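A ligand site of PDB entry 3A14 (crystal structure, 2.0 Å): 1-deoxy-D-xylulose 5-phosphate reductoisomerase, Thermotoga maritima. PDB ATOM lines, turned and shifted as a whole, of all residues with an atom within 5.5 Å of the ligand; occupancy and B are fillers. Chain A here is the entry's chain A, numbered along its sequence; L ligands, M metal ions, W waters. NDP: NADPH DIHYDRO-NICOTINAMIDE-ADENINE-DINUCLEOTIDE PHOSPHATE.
The backbone carbonyl oxygen (O) of Ser 94 sits at hydrogen-bond distance from the side-chain hydroxyl (OG) of Ser 97. N of Gly 10 sits at hydrogen-bond distance from OG of Ser 35 (2.9 Å). The side-chain amino group (NZ) of Lys 117 lies close to the side-chain carboxylate (OE2) of Glu 209. OG of Ser 14 lies within hydrogen-bond range of OE1 of Gln 18, 3.1 Å away. N of Glu 118 is in hydrogen-bond range of OD1 of Asn 116 (3.1 Å). The backbone NH of Ala 115 sits at hydrogen-bond distance from the backbone carbonyl oxygen of Val 91, 2.9 Å away. The backbone NH (N) of Ala 11 is in hydrogen-bond range of the backbone carbonyl oxygen (O) of Ser 35 (2.9 Å). The backbone NH (N) of Thr 58 sits at hydrogen-bond distance from the backbone carbonyl oxygen (O) of Phe 36 (3.2 Å).
N of His 37 lies within hydrogen-bond range of O2X of the ligand (3.0 Å). A nitrogen (N1A) of the ligand is in hydrogen-bond range of the side-chain hydroxyl (OG) of Ser 97 (3.1 Å). The backbone NH of Ile 15 sits at hydrogen-bond distance from an oxygen (O2N) of the ligand (3.0 Å). N of Lys 117 lies within hydrogen-bond range of O3D of the ligand, 3.3 Å away. OG1 of Thr 12 sits at hydrogen-bond distance from O3B of the ligand. The backbone NH (N) of Thr 12 sits at hydrogen-bond distance from an oxygen (O3B) of the ligand (3.3 Å). The backbone NH (N) of Ser 14 is in hydrogen-bond range of an oxygen (O2A) of the ligand (3.1 Å). The backbone carbonyl oxygen (O) of Gly 10 lies close to an oxygen (O3B) of the ligand, at 3.4 Å. An oxygen (O3B) of the ligand is in hydrogen-bond range of the backbone NH (N) of Gly 13 (3.3 Å). The backbone NH (N) of Asn 39 is in hydrogen-bond range of an oxygen (O2X) of the ligand (2.7 Å). An oxygen (O4D) of the ligand sits close to the backbone carbonyl oxygen (O) of Ala 115, 2.4 Å away. O4B of the ligand lies within hydrogen-bond range of N of Ser 94. OE1 of Glu 118 sits at hydrogen-bond distance from O3D of the ligand. OG of Ser 38 sits at hydrogen-bond distance from O3X of the ligand (3.2 Å). An oxygen (O2X) of the ligand lies within hydrogen-bond range of the backbone NH (N) of Ser 38. OG1 of Thr 58 sits close to N3A of the ligand (3.4 Å).
N of Ala 11 touches O3B of the ligand, 3.8 Å away. CD1 of Phe 36 touches O2X of the ligand, at 3.9 Å. Ala 92 touches the ligand. Val 93 touches the ligand. Asn 116 touches the ligand (CA to O3D, 3.5 Å). OD1 of Asp 142 touches C5N of the ligand (3.5 Å). CD1 of Ile 196 touches O1N of the ligand, 3.2 Å away. Met 254 touches the ligand. Hydrophobic or aromatic side chains that line the ligand: Ile 15, Phe 36, His 37, Val 93, Ala 115, Ile 196 and Met 254. 22 residues have an atom within 4 Å of the ligand: Gly 10, Ala 11, Thr 12, Gly 13, Ser 14, Ile 15, Phe 36, His 37, Ser 38, Asn 39, Thr 58, Ala 92, Val 93, Ser 94, Ser 97, Ala 115, Asn 116, Lys 117, Glu 118, Asp 142, Ile 196 and Met 254. Along chain A the residues within 4 Å of the ligand span positions 10 to 254.
Water W2 lies within hydrogen-bond range of N3A of the ligand (2.8 Å), OG of Ser 35 (2.9 Å) and OG1 of Thr 58 (3.3 Å). Water W5 lies within hydrogen-bond range of the side-chain amide nitrogen (ND2) of Asn 39 (2.7 Å), an oxygen (O1X) of the ligand (2.8 Å) and the backbone carbonyl oxygen (O) of Thr 12 (2.9 Å). Water W3 lies within hydrogen-bond range of OG of Ser 97 (2.5 Å), O of Ser 94 (2.9 Å) and N6A of the ligand (2.9 Å). Water W1 lies within hydrogen-bond range of the side-chain amide nitrogen (ND2) of Asn 205 and the side-chain amino group (NZ) of Lys 117. Water W4 lies within hydrogen-bond range of the backbone NH (N) of Ser 143 and the side-chain sulfur (SD) of Met 254.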
ATOM      1  N   GLY A  10     -16.178  28.359  17.446  1.00  0.00           N
ATOM      2  CA  GLY A  10     -16.752  27.254  18.178  1.00  0.00           C
ATOM      3  C   GLY A  10     -15.631  26.351  18.712  1.00  0.00           C
ATOM      4  O   GLY A  10     -15.713  25.122  18.595  1.00  0.00           O
ATOM      5  N   ALA A  11     -14.611  26.963  19.293  1.00  0.00           N
ATOM      6  CA  ALA A  11     -13.421  26.239  19.774  1.00  0.00           C
ATOM      7  C   ALA A  11     -13.672  25.263  20.924  1.00  0.00           C
ATOM      8  O   ALA A  11     -12.865  24.329  21.172  1.00  0.00           O
ATOM      9  CB  ALA A  11     -12.324  27.221  20.164  1.00  0.00           C
ATOM     10  N   THR A  12     -14.808  25.442  21.607  1.00  0.00           N
ATOM     11  CA  THR A  12     -15.074  24.699  22.821  1.00  0.00           C
ATOM     12  C   THR A  12     -15.931  23.474  22.574  1.00  0.00           C
ATOM     13  O   THR A  12     -16.214  22.722  23.511  1.00  0.00           O
ATOM     14  CB  THR A  12     -15.746  25.587  23.889  1.00  0.00           C
ATOM     15  OG1 THR A  12     -16.899  26.210  23.310  1.00  0.00           O
ATOM     16  CG2 THR A  12     -14.782  26.663  24.401  1.00  0.00           C
ATOM     17  N   GLY A  13     -16.336  23.255  21.322  1.00  0.00           N
ATOM     18  CA  GLY A  13     -17.121  22.088  20.970  1.00  0.00           C
ATOM     19  C   GLY A  13     -16.235  20.915  20.561  1.00  0.00           C
ATOM     20  O   GLY A  13     -15.007  20.975  20.624  1.00  0.00           O
ATOM     21  N   SER A  14     -16.887  19.846  20.133  1.00  0.00           N
ATOM     22  CA  SER A  14     -16.207  18.605  19.723  1.00  0.00           C
ATOM     23  C   SER A  14     -15.211  18.795  18.574  1.00  0.00           C
ATOM     24  O   SER A  14     -14.034  18.427  18.696  1.00  0.00           O
ATOM     25  CB  SER A  14     -17.280  17.575  19.327  1.00  0.00           C
ATOM     26  OG  SER A  14     -16.649  16.355  18.982  1.00  0.00           O
ATOM     27  N   ILE A  15     -15.662  19.383  17.458  1.00  0.00           N
ATOM     28  CA  ILE A  15     -14.761  19.631  16.320  1.00  0.00           C
ATOM     29  C   ILE A  15     -13.659  20.623  16.727  1.00  0.00           C
ATOM     30  O   ILE A  15     -12.481  20.447  16.378  1.00  0.00           O
ATOM     31  CB  ILE A  15     -15.548  20.080  15.060  1.00  0.00           C
ATOM     32  CG1 ILE A  15     -16.394  18.891  14.537  1.00  0.00           C
ATOM     33  CG2 ILE A  15     -14.612  20.628  13.941  1.00  0.00           C
ATOM     34  CD1 ILE A  15     -15.564  17.691  14.102  1.00  0.00           C
ATOM     35  N   GLY A  16     -14.046  21.630  17.499  1.00  0.00           N
ATOM     36  CA  GLY A  16     -13.087  22.653  17.948  1.00  0.00           C
ATOM     37  C   GLY A  16     -11.950  22.042  18.705  1.00  0.00           C
ATOM     38  O   GLY A  16     -10.805  22.278  18.369  1.00  0.00           O
ATOM     39  N   GLN A  18     -11.097  18.782  18.910  1.00  0.00           N
ATOM     40  CA  GLN A  18     -10.383  17.855  18.043  1.00  0.00           C
ATOM     41  C   GLN A  18      -9.388  18.595  17.106  1.00  0.00           C
ATOM     42  O   GLN A  18      -8.276  18.107  16.874  1.00  0.00           O
ATOM     43  CB  GLN A  18     -11.346  16.959  17.282  1.00  0.00           C
ATOM     44  CG  GLN A  18     -11.991  15.869  18.173  1.00  0.00           C
ATOM     45  CD  GLN A  18     -13.030  15.053  17.427  1.00  0.00           C
ATOM     46  OE1 GLN A  18     -14.205  15.404  17.374  1.00  0.00           O
ATOM     47  NE2 GLN A  18     -12.599  13.957  16.836  1.00  0.00           N
ATOM     48  N   SER A  35     -13.501  31.654  18.680  1.00  0.00           N
ATOM     49  CA  SER A  35     -14.793  32.073  19.215  1.00  0.00           C
ATOM     50  C   SER A  35     -15.332  30.937  20.062  1.00  0.00           C
ATOM     51  O   SER A  35     -15.015  29.757  19.833  1.00  0.00           O
ATOM     52  CB  SER A  35     -15.761  32.415  18.089  1.00  0.00           C
ATOM     53  OG  SER A  35     -16.415  31.280  17.580  1.00  0.00           O
ATOM     54  N   PHE A  36     -16.163  31.261  21.051  1.00  0.00           N
ATOM     55  CA  PHE A  36     -16.865  30.238  21.815  1.00  0.00           C
ATOM     56  C   PHE A  36     -18.144  30.871  22.342  1.00  0.00           C
ATOM     57  O   PHE A  36     -18.274  32.101  22.300  1.00  0.00           O
ATOM     58  CB  PHE A  36     -15.989  29.717  22.967  1.00  0.00           C
ATOM     59  CG  PHE A  36     -15.827  30.701  24.099  1.00  0.00           C
ATOM     60  CD1 PHE A  36     -16.612  30.594  25.238  1.00  0.00           C
ATOM     61  CD2 PHE A  36     -14.891  31.717  24.030  1.00  0.00           C
ATOM     62  CE1 PHE A  36     -16.470  31.489  26.284  1.00  0.00           C
ATOM     63  CE2 PHE A  36     -14.747  32.617  25.085  1.00  0.00           C
ATOM     64  CZ  PHE A  36     -15.550  32.500  26.200  1.00  0.00           C
ATOM     65  N   HIS A  37     -19.086  30.053  22.815  1.00  0.00           N
ATOM     66  CA  HIS A  37     -20.404  30.590  23.146  1.00  0.00           C
ATOM     67  C   HIS A  37     -20.605  30.882  24.642  1.00  0.00           C
ATOM     68  O   HIS A  37     -20.739  32.038  25.041  1.00  0.00           O
ATOM     69  CB  HIS A  37     -21.518  29.708  22.583  1.00  0.00           C
ATOM     70  CG  HIS A  37     -22.871  30.358  22.645  1.00  0.00           C
ATOM     71  ND1 HIS A  37     -23.881  29.915  23.464  1.00  0.00           N
ATOM     72  CD2 HIS A  37     -23.365  31.441  21.991  1.00  0.00           C
ATOM     73  CE1 HIS A  37     -24.934  30.695  23.327  1.00  0.00           C
ATOM     74  NE2 HIS A  37     -24.645  31.630  22.427  1.00  0.00           N
ATOM     75  N   SER A  38     -20.599  29.841  25.469  1.00  0.00           N
ATOM     76  CA  SER A  38     -20.741  30.020  26.915  1.00  0.00           C
ATOM     77  C   SER A  38     -19.694  29.272  27.780  1.00  0.00           C
ATOM     78  O   SER A  38     -19.476  29.655  28.940  1.00  0.00           O
ATOM     79  CB  SER A  38     -22.149  29.616  27.351  1.00  0.00           C
ATOM     80  OG  SER A  38     -22.323  28.215  27.160  1.00  0.00           O
ATOM     81  N   ASN A  39     -19.062  28.209  27.247  1.00  0.00           N
ATOM     82  CA  ASN A  39     -18.114  27.412  28.053  1.00  0.00           C
ATOM     83  C   ASN A  39     -16.787  28.103  28.380  1.00  0.00           C
ATOM     84  O   ASN A  39     -15.742  27.788  27.807  1.00  0.00           O
ATOM     85  CB  ASN A  39     -17.854  26.040  27.402  1.00  0.00           C
ATOM     86  CG  ASN A  39     -17.238  25.039  28.376  1.00  0.00           C
ATOM     87  OD1 ASN A  39     -16.675  25.420  29.399  1.00  0.00           O
ATOM     88  ND2 ASN A  39     -17.338  23.770  28.061  1.00  0.00           N
ATOM     89  N   LEU A  40     -16.838  29.030  29.339  1.00  0.00           N
ATOM     90  CA  LEU A  40     -15.683  29.841  29.737  1.00  0.00           C
ATOM     91  C   LEU A  40     -14.522  29.063  30.402  1.00  0.00           C
ATOM     92  O   LEU A  40     -13.367  29.394  30.212  1.00  0.00           O
ATOM     93  CB  LEU A  40     -16.153  31.027  30.614  1.00  0.00           C
ATOM     94  CG  LEU A  40     -17.483  30.794  31.358  1.00  0.00           C
ATOM     95  CD1 LEU A  40     -17.361  29.691  32.435  1.00  0.00           C
ATOM     96  CD2 LEU A  40     -18.044  32.078  31.992  1.00  0.00           C
ATOM     97  N   THR A  58     -19.786  34.860  21.774  1.00  0.00           N
ATOM     98  CA  THR A  58     -21.030  34.896  21.036  1.00  0.00           C
ATOM     99  C   THR A  58     -22.216  34.760  21.965  1.00  0.00           C
ATOM    100  O   THR A  58     -23.333  35.114  21.590  1.00  0.00           O
ATOM    101  CB  THR A  58     -21.084  33.834  19.889  1.00  0.00           C
ATOM    102  OG1 THR A  58     -20.971  32.507  20.425  1.00  0.00           O
ATOM    103  CG2 THR A  58     -19.974  34.094  18.854  1.00  0.00           C
ATOM    104  N   VAL A  91     -14.766  26.571  10.801  1.00  0.00           N
ATOM    105  CA  VAL A  91     -16.108  27.030  11.246  1.00  0.00           C
ATOM    106  C   VAL A  91     -16.824  25.874  11.934  1.00  0.00           C
ATOM    107  O   VAL A  91     -17.419  25.015  11.270  1.00  0.00           O
ATOM    108  CB  VAL A  91     -16.992  27.584  10.102  1.00  0.00           C
ATOM    109  CG1 VAL A  91     -18.363  28.046  10.650  1.00  0.00           C
ATOM    110  CG2 VAL A  91     -16.298  28.731   9.354  1.00  0.00           C
ATOM    111  N   ALA A  92     -16.724  25.820  13.242  1.00  0.00           N
ATOM    112  CA  ALA A  92     -17.271  24.677  13.963  1.00  0.00           C
ATOM    113  C   ALA A  92     -18.312  25.124  14.976  1.00  0.00           C
ATOM    114  O   ALA A  92     -18.519  24.461  16.003  1.00  0.00           O
ATOM    115  CB  ALA A  92     -16.148  23.883  14.626  1.00  0.00           C
ATOM    116  N   VAL A  93     -18.980  26.227  14.668  1.00  0.00           N
ATOM    117  CA  VAL A  93     -20.091  26.687  15.504  1.00  0.00           C
ATOM    118  C   VAL A  93     -21.271  25.744  15.287  1.00  0.00           C
ATOM    119  O   VAL A  93     -21.433  25.193  14.193  1.00  0.00           O
ATOM    120  CB  VAL A  93     -20.491  28.167  15.227  1.00  0.00           C
ATOM    121  CG1 VAL A  93     -19.318  29.105  15.582  1.00  0.00           C
ATOM    122  CG2 VAL A  93     -20.872  28.371  13.806  1.00  0.00           C
ATOM    123  N   SER A  94     -22.060  25.516  16.317  1.00  0.00           N
ATOM    124  CA  SER A  94     -23.235  24.666  16.128  1.00  0.00           C
ATOM    125  C   SER A  94     -24.462  25.528  15.893  1.00  0.00           C
ATOM    126  O   SER A  94     -24.544  26.655  16.363  1.00  0.00           O
ATOM    127  CB  SER A  94     -23.490  23.750  17.330  1.00  0.00           C
ATOM    128  OG  SER A  94     -23.929  24.536  18.415  1.00  0.00           O
ATOM    129  N   GLY A  95     -25.408  24.970  15.148  1.00  0.00           N
ATOM    130  CA  GLY A  95     -26.732  25.562  15.005  1.00  0.00           C
ATOM    131  C   GLY A  95     -26.800  26.608  13.919  1.00  0.00           C
ATOM    132  O   GLY A  95     -25.886  26.756  13.098  1.00  0.00           O
ATOM    133  N   SER A  97     -26.594  29.801  13.905  1.00  0.00           N
ATOM    134  CA  SER A  97     -25.616  30.893  13.876  1.00  0.00           C
ATOM    135  C   SER A  97     -24.461  30.569  12.911  1.00  0.00           C
ATOM    136  O   SER A  97     -23.689  31.448  12.532  1.00  0.00           O
ATOM    137  CB  SER A  97     -25.047  31.102  15.272  1.00  0.00           C
ATOM    138  OG  SER A  97     -24.595  29.824  15.727  1.00  0.00           O
ATOM    139  N   ALA A 115     -17.376  23.012   9.144  1.00  0.00           N
ATOM    140  CA  ALA A 115     -18.004  22.031  10.039  1.00  0.00           C
ATOM    141  C   ALA A 115     -19.234  22.639  10.697  1.00  0.00           C
ATOM    142  O   ALA A 115     -19.365  22.652  11.934  1.00  0.00           O
ATOM    143  CB  ALA A 115     -17.031  21.596  11.121  1.00  0.00           C
ATOM    144  N   ASN A 116     -20.084  23.256   9.902  1.00  0.00           N
ATOM    145  CA  ASN A 116     -21.398  23.640  10.356  1.00  0.00           C
ATOM    146  C   ASN A 116     -22.303  23.305   9.204  1.00  0.00           C
ATOM    147  O   ASN A 116     -22.053  23.761   8.089  1.00  0.00           O
ATOM    148  CB  ASN A 116     -21.522  25.127  10.644  1.00  0.00           C
ATOM    149  CG  ASN A 116     -22.956  25.512  10.994  1.00  0.00           C
ATOM    150  OD1 ASN A 116     -23.758  25.791  10.102  1.00  0.00           O
ATOM    151  ND2 ASN A 116     -23.295  25.489  12.297  1.00  0.00           N
ATOM    152  N   LYS A 117     -23.330  22.523   9.492  1.00  0.00           N
ATOM    153  CA  LYS A 117     -24.265  22.029   8.477  1.00  0.00           C
ATOM    154  C   LYS A 117     -25.398  23.008   8.143  1.00  0.00           C
ATOM    155  O   LYS A 117     -25.853  23.065   6.988  1.00  0.00           O
ATOM    156  CB  LYS A 117     -24.886  20.709   8.941  1.00  0.00           C
ATOM    157  CG  LYS A 117     -23.859  19.620   9.253  1.00  0.00           C
ATOM    158  CD  LYS A 117     -24.496  18.224   9.117  1.00  0.00           C
ATOM    159  CE  LYS A 117     -23.509  17.141   9.438  1.00  0.00           C
ATOM    160  NZ  LYS A 117     -22.407  17.123   8.447  1.00  0.00           N
ATOM    161  N   GLU A 118     -25.862  23.755   9.140  1.00  0.00           N
ATOM    162  CA  GLU A 118     -27.009  24.672   8.967  1.00  0.00           C
ATOM    163  C   GLU A 118     -26.771  25.678   7.874  1.00  0.00           C
ATOM    164  O   GLU A 118     -27.692  26.043   7.153  1.00  0.00           O
ATOM    165  CB  GLU A 118     -27.354  25.401  10.282  1.00  0.00           C
ATOM    166  CG  GLU A 118     -28.089  24.510  11.340  1.00  0.00           C
ATOM    167  CD  GLU A 118     -27.174  23.465  12.001  1.00  0.00           C
ATOM    168  OE1 GLU A 118     -25.930  23.533  11.825  1.00  0.00           O
ATOM    169  OE2 GLU A 118     -27.715  22.558  12.692  1.00  0.00           O
ATOM    170  N   VAL A 141     -15.359  19.631   6.403  1.00  0.00           N
ATOM    171  CA  VAL A 141     -14.719  18.868   7.484  1.00  0.00           C
ATOM    172  C   VAL A 141     -15.508  17.563   7.754  1.00  0.00           C
ATOM    173  O   VAL A 141     -14.950  16.575   8.223  1.00  0.00           O
ATOM    174  CB  VAL A 141     -14.533  19.747   8.764  1.00  0.00           C
ATOM    175  CG1 VAL A 141     -14.049  18.931   9.940  1.00  0.00           C
ATOM    176  CG2 VAL A 141     -13.550  20.879   8.482  1.00  0.00           C
ATOM    177  N   ASP A 142     -16.799  17.555   7.466  1.00  0.00           N
ATOM    178  CA  ASP A 142     -17.637  16.349   7.659  1.00  0.00           C
ATOM    179  C   ASP A 142     -16.959  15.153   7.020  1.00  0.00           C
ATOM    180  O   ASP A 142     -16.483  15.280   5.912  1.00  0.00           O
ATOM    181  CB  ASP A 142     -18.987  16.605   6.986  1.00  0.00           C
ATOM    182  CG  ASP A 142     -19.901  15.410   7.054  1.00  0.00           C
ATOM    183  OD1 ASP A 142     -20.602  15.251   8.075  1.00  0.00           O
ATOM    184  OD2 ASP A 142     -19.932  14.654   6.059  1.00  0.00           O
ATOM    185  N   SER A 143     -16.919  13.995   7.687  1.00  0.00           N
ATOM    186  CA  SER A 143     -16.127  12.880   7.215  1.00  0.00           C
ATOM    187  C   SER A 143     -16.617  12.364   5.873  1.00  0.00           C
ATOM    188  O   SER A 143     -15.810  11.985   5.031  1.00  0.00           O
ATOM    189  CB  SER A 143     -16.106  11.745   8.259  1.00  0.00           C
ATOM    190  OG  SER A 143     -17.384  11.124   8.297  1.00  0.00           O
ATOM    191  N   ILE A 196     -26.291  15.620  17.823  1.00  0.00           N
ATOM    192  CA  ILE A 196     -25.754  14.846  16.722  1.00  0.00           C
ATOM    193  C   ILE A 196     -26.142  13.389  16.875  1.00  0.00           C
ATOM    194  O   ILE A 196     -26.560  12.737  15.912  1.00  0.00           O
ATOM    195  CB  ILE A 196     -24.214  15.008  16.586  1.00  0.00           C
ATOM    196  CG1 ILE A 196     -23.912  16.328  15.880  1.00  0.00           C
ATOM    197  CG2 ILE A 196     -23.596  13.840  15.818  1.00  0.00           C
ATOM    198  CD1 ILE A 196     -22.581  16.945  16.283  1.00  0.00           C
ATOM    199  N   ASN A 205     -29.569  13.783  10.528  1.00  0.00           N
ATOM    200  CA  ASN A 205     -28.185  14.203  10.198  1.00  0.00           C
ATOM    201  C   ASN A 205     -27.797  13.808   8.772  1.00  0.00           C
ATOM    202  O   ASN A 205     -27.139  14.573   8.065  1.00  0.00           O
ATOM    203  CB  ASN A 205     -27.194  13.613  11.184  1.00  0.00           C
ATOM    204  CG  ASN A 205     -25.820  14.215  11.029  1.00  0.00           C
ATOM    205  OD1 ASN A 205     -25.603  15.392  11.346  1.00  0.00           O
ATOM    206  ND2 ASN A 205     -24.886  13.418  10.519  1.00  0.00           N
ATOM    207  N   GLU A 209     -26.773  15.995   5.416  1.00  0.00           N
ATOM    208  CA  GLU A 209     -25.578  15.697   4.615  1.00  0.00           C
ATOM    209  C   GLU A 209     -25.863  15.569   3.126  1.00  0.00           C
ATOM    210  O   GLU A 209     -25.040  15.971   2.296  1.00  0.00           O
ATOM    211  CB  GLU A 209     -24.841  14.469   5.152  1.00  0.00           C
ATOM    212  CG  GLU A 209     -24.223  14.705   6.517  1.00  0.00           C
ATOM    213  CD  GLU A 209     -23.468  13.476   7.023  1.00  0.00           C
ATOM    214  OE1 GLU A 209     -23.521  12.429   6.360  1.00  0.00           O
ATOM    215  OE2 GLU A 209     -22.794  13.557   8.087  1.00  0.00           O
ATOM    216  N   MET A 254     -12.559  11.909  13.608  1.00  0.00           N
ATOM    217  CA  MET A 254     -12.761  13.217  12.932  1.00  0.00           C
ATOM    218  C   MET A 254     -11.471  13.997  12.786  1.00  0.00           C
ATOM    219  O   MET A 254     -11.424  14.959  12.011  1.00  0.00           O
ATOM    220  CB  MET A 254     -13.812  14.054  13.674  1.00  0.00           C
ATOM    221  CG  MET A 254     -15.283  13.651  13.422  1.00  0.00           C
ATOM    222  SD  MET A 254     -15.700  13.571  11.672  1.00  0.00           S
ATOM    223  CE  MET A 254     -15.516  15.280  11.129  1.00  0.00           C
HETATM  224  PA  NDP L   1     -20.760  21.299  19.798  1.00  0.00           P
HETATM  225  O1A NDP L   1     -22.072  21.589  20.462  1.00  0.00           O
HETATM  226  O2A NDP L   1     -19.932  20.052  20.435  1.00  0.00           O
HETATM  227  O5B NDP L   1     -19.831  22.642  19.771  1.00  0.00           O
HETATM  228  C5B NDP L   1     -20.110  23.703  18.843  1.00  0.00           C
HETATM  229  C4B NDP L   1     -19.495  25.063  19.248  1.00  0.00           C
HETATM  230  O4B NDP L   1     -20.443  26.129  18.862  1.00  0.00           O
HETATM  231  C3B NDP L   1     -19.188  25.280  20.750  1.00  0.00           C
HETATM  232  O3B NDP L   1     -17.983  26.084  20.883  1.00  0.00           O
HETATM  233  C2B NDP L   1     -20.347  26.118  21.228  1.00  0.00           C
HETATM  234  O2B NDP L   1     -19.905  26.975  22.304  1.00  0.00           O
HETATM  235  C1B NDP L   1     -20.567  26.999  19.999  1.00  0.00           C
HETATM  236  N9A NDP L   1     -21.931  27.589  19.967  1.00  0.00           N
HETATM  237  C8A NDP L   1     -23.029  27.054  20.520  1.00  0.00           C
HETATM  238  N7A NDP L   1     -24.062  27.866  20.273  1.00  0.00           N
HETATM  239  C5A NDP L   1     -23.609  28.914  19.590  1.00  0.00           C
HETATM  240  C6A NDP L   1     -24.217  30.048  19.077  1.00  0.00           C
HETATM  241  N6A NDP L   1     -25.533  30.223  19.256  1.00  0.00           N
HETATM  242  N1A NDP L   1     -23.466  30.937  18.411  1.00  0.00           N
HETATM  243  C2A NDP L   1     -22.152  30.756  18.224  1.00  0.00           C
HETATM  244  N3A NDP L   1     -21.540  29.675  18.705  1.00  0.00           N
HETATM  245  C4A NDP L   1     -22.251  28.744  19.382  1.00  0.00           C
HETATM  246  O3  NDP L   1     -20.997  20.949  18.216  1.00  0.00           O
HETATM  247  PN  NDP L   1     -19.965  20.059  17.295  1.00  0.00           P
HETATM  248  O1N NDP L   1     -20.107  18.603  17.533  1.00  0.00           O
HETATM  249  O2N NDP L   1     -18.410  20.575  17.382  1.00  0.00           O
HETATM  250  O5D NDP L   1     -20.420  20.473  15.789  1.00  0.00           O
HETATM  251  C5D NDP L   1     -20.652  21.824  15.350  1.00  0.00           C
HETATM  252  C4D NDP L   1     -21.115  21.781  13.894  1.00  0.00           C
HETATM  253  O4D NDP L   1     -20.195  20.807  13.263  1.00  0.00           O
HETATM  254  C3D NDP L   1     -22.546  21.215  13.747  1.00  0.00           C
HETATM  255  O3D NDP L   1     -23.275  21.923  12.715  1.00  0.00           O
HETATM  256  C2D NDP L   1     -22.277  19.751  13.350  1.00  0.00           C
HETATM  257  O2D NDP L   1     -23.338  19.181  12.577  1.00  0.00           O
HETATM  258  C1D NDP L   1     -21.000  19.871  12.508  1.00  0.00           C
HETATM  259  N1N NDP L   1     -20.368  18.538  12.420  1.00  0.00           N
HETATM  260  C2N NDP L   1     -20.032  17.848  13.595  1.00  0.00           C
HETATM  261  C3N NDP L   1     -19.459  16.580  13.524  1.00  0.00           C
HETATM  262  C7N NDP L   1     -19.104  15.842  14.818  1.00  0.00           C
HETATM  263  O7N NDP L   1     -18.592  14.722  14.778  1.00  0.00           O
HETATM  264  N7N NDP L   1     -19.385  16.484  15.958  1.00  0.00           N
HETATM  265  C4N NDP L   1     -19.163  15.914  12.153  1.00  0.00           C
HETATM  266  C5N NDP L   1     -19.533  16.694  11.044  1.00  0.00           C
HETATM  267  C6N NDP L   1     -20.120  17.967  11.153  1.00  0.00           C
HETATM  268  P2B NDP L   1     -20.013  26.545  23.886  1.00  0.00           P
HETATM  269  O1X NDP L   1     -19.626  25.145  24.169  1.00  0.00           O
HETATM  270  O2X NDP L   1     -19.109  27.634  24.651  1.00  0.00           O
HETATM  271  O3X NDP L   1     -21.506  26.831  24.396  1.00  0.00           O
HETATM  272 MG    MG M   1     -21.003  12.988   8.734  1.00  0.00          MG
HETATM  273  O   HOH W   1     -21.673  14.521  10.618  1.00  0.00           O
HETATM  274  O   HOH W   2     -18.905  30.532  18.826  1.00  0.00           O
HETATM  275  O   HOH W   3     -26.516  28.744  16.916  1.00  0.00           O
HETATM  276  O   HOH W   4     -18.709  13.591  10.124  1.00  0.00           O
HETATM  277  O   HOH W   5     -18.129  23.202  25.575  1.00  0.00           O
HETATM  278  O   HOH W   6     -16.649  22.546  17.919  1.00  0.00           O
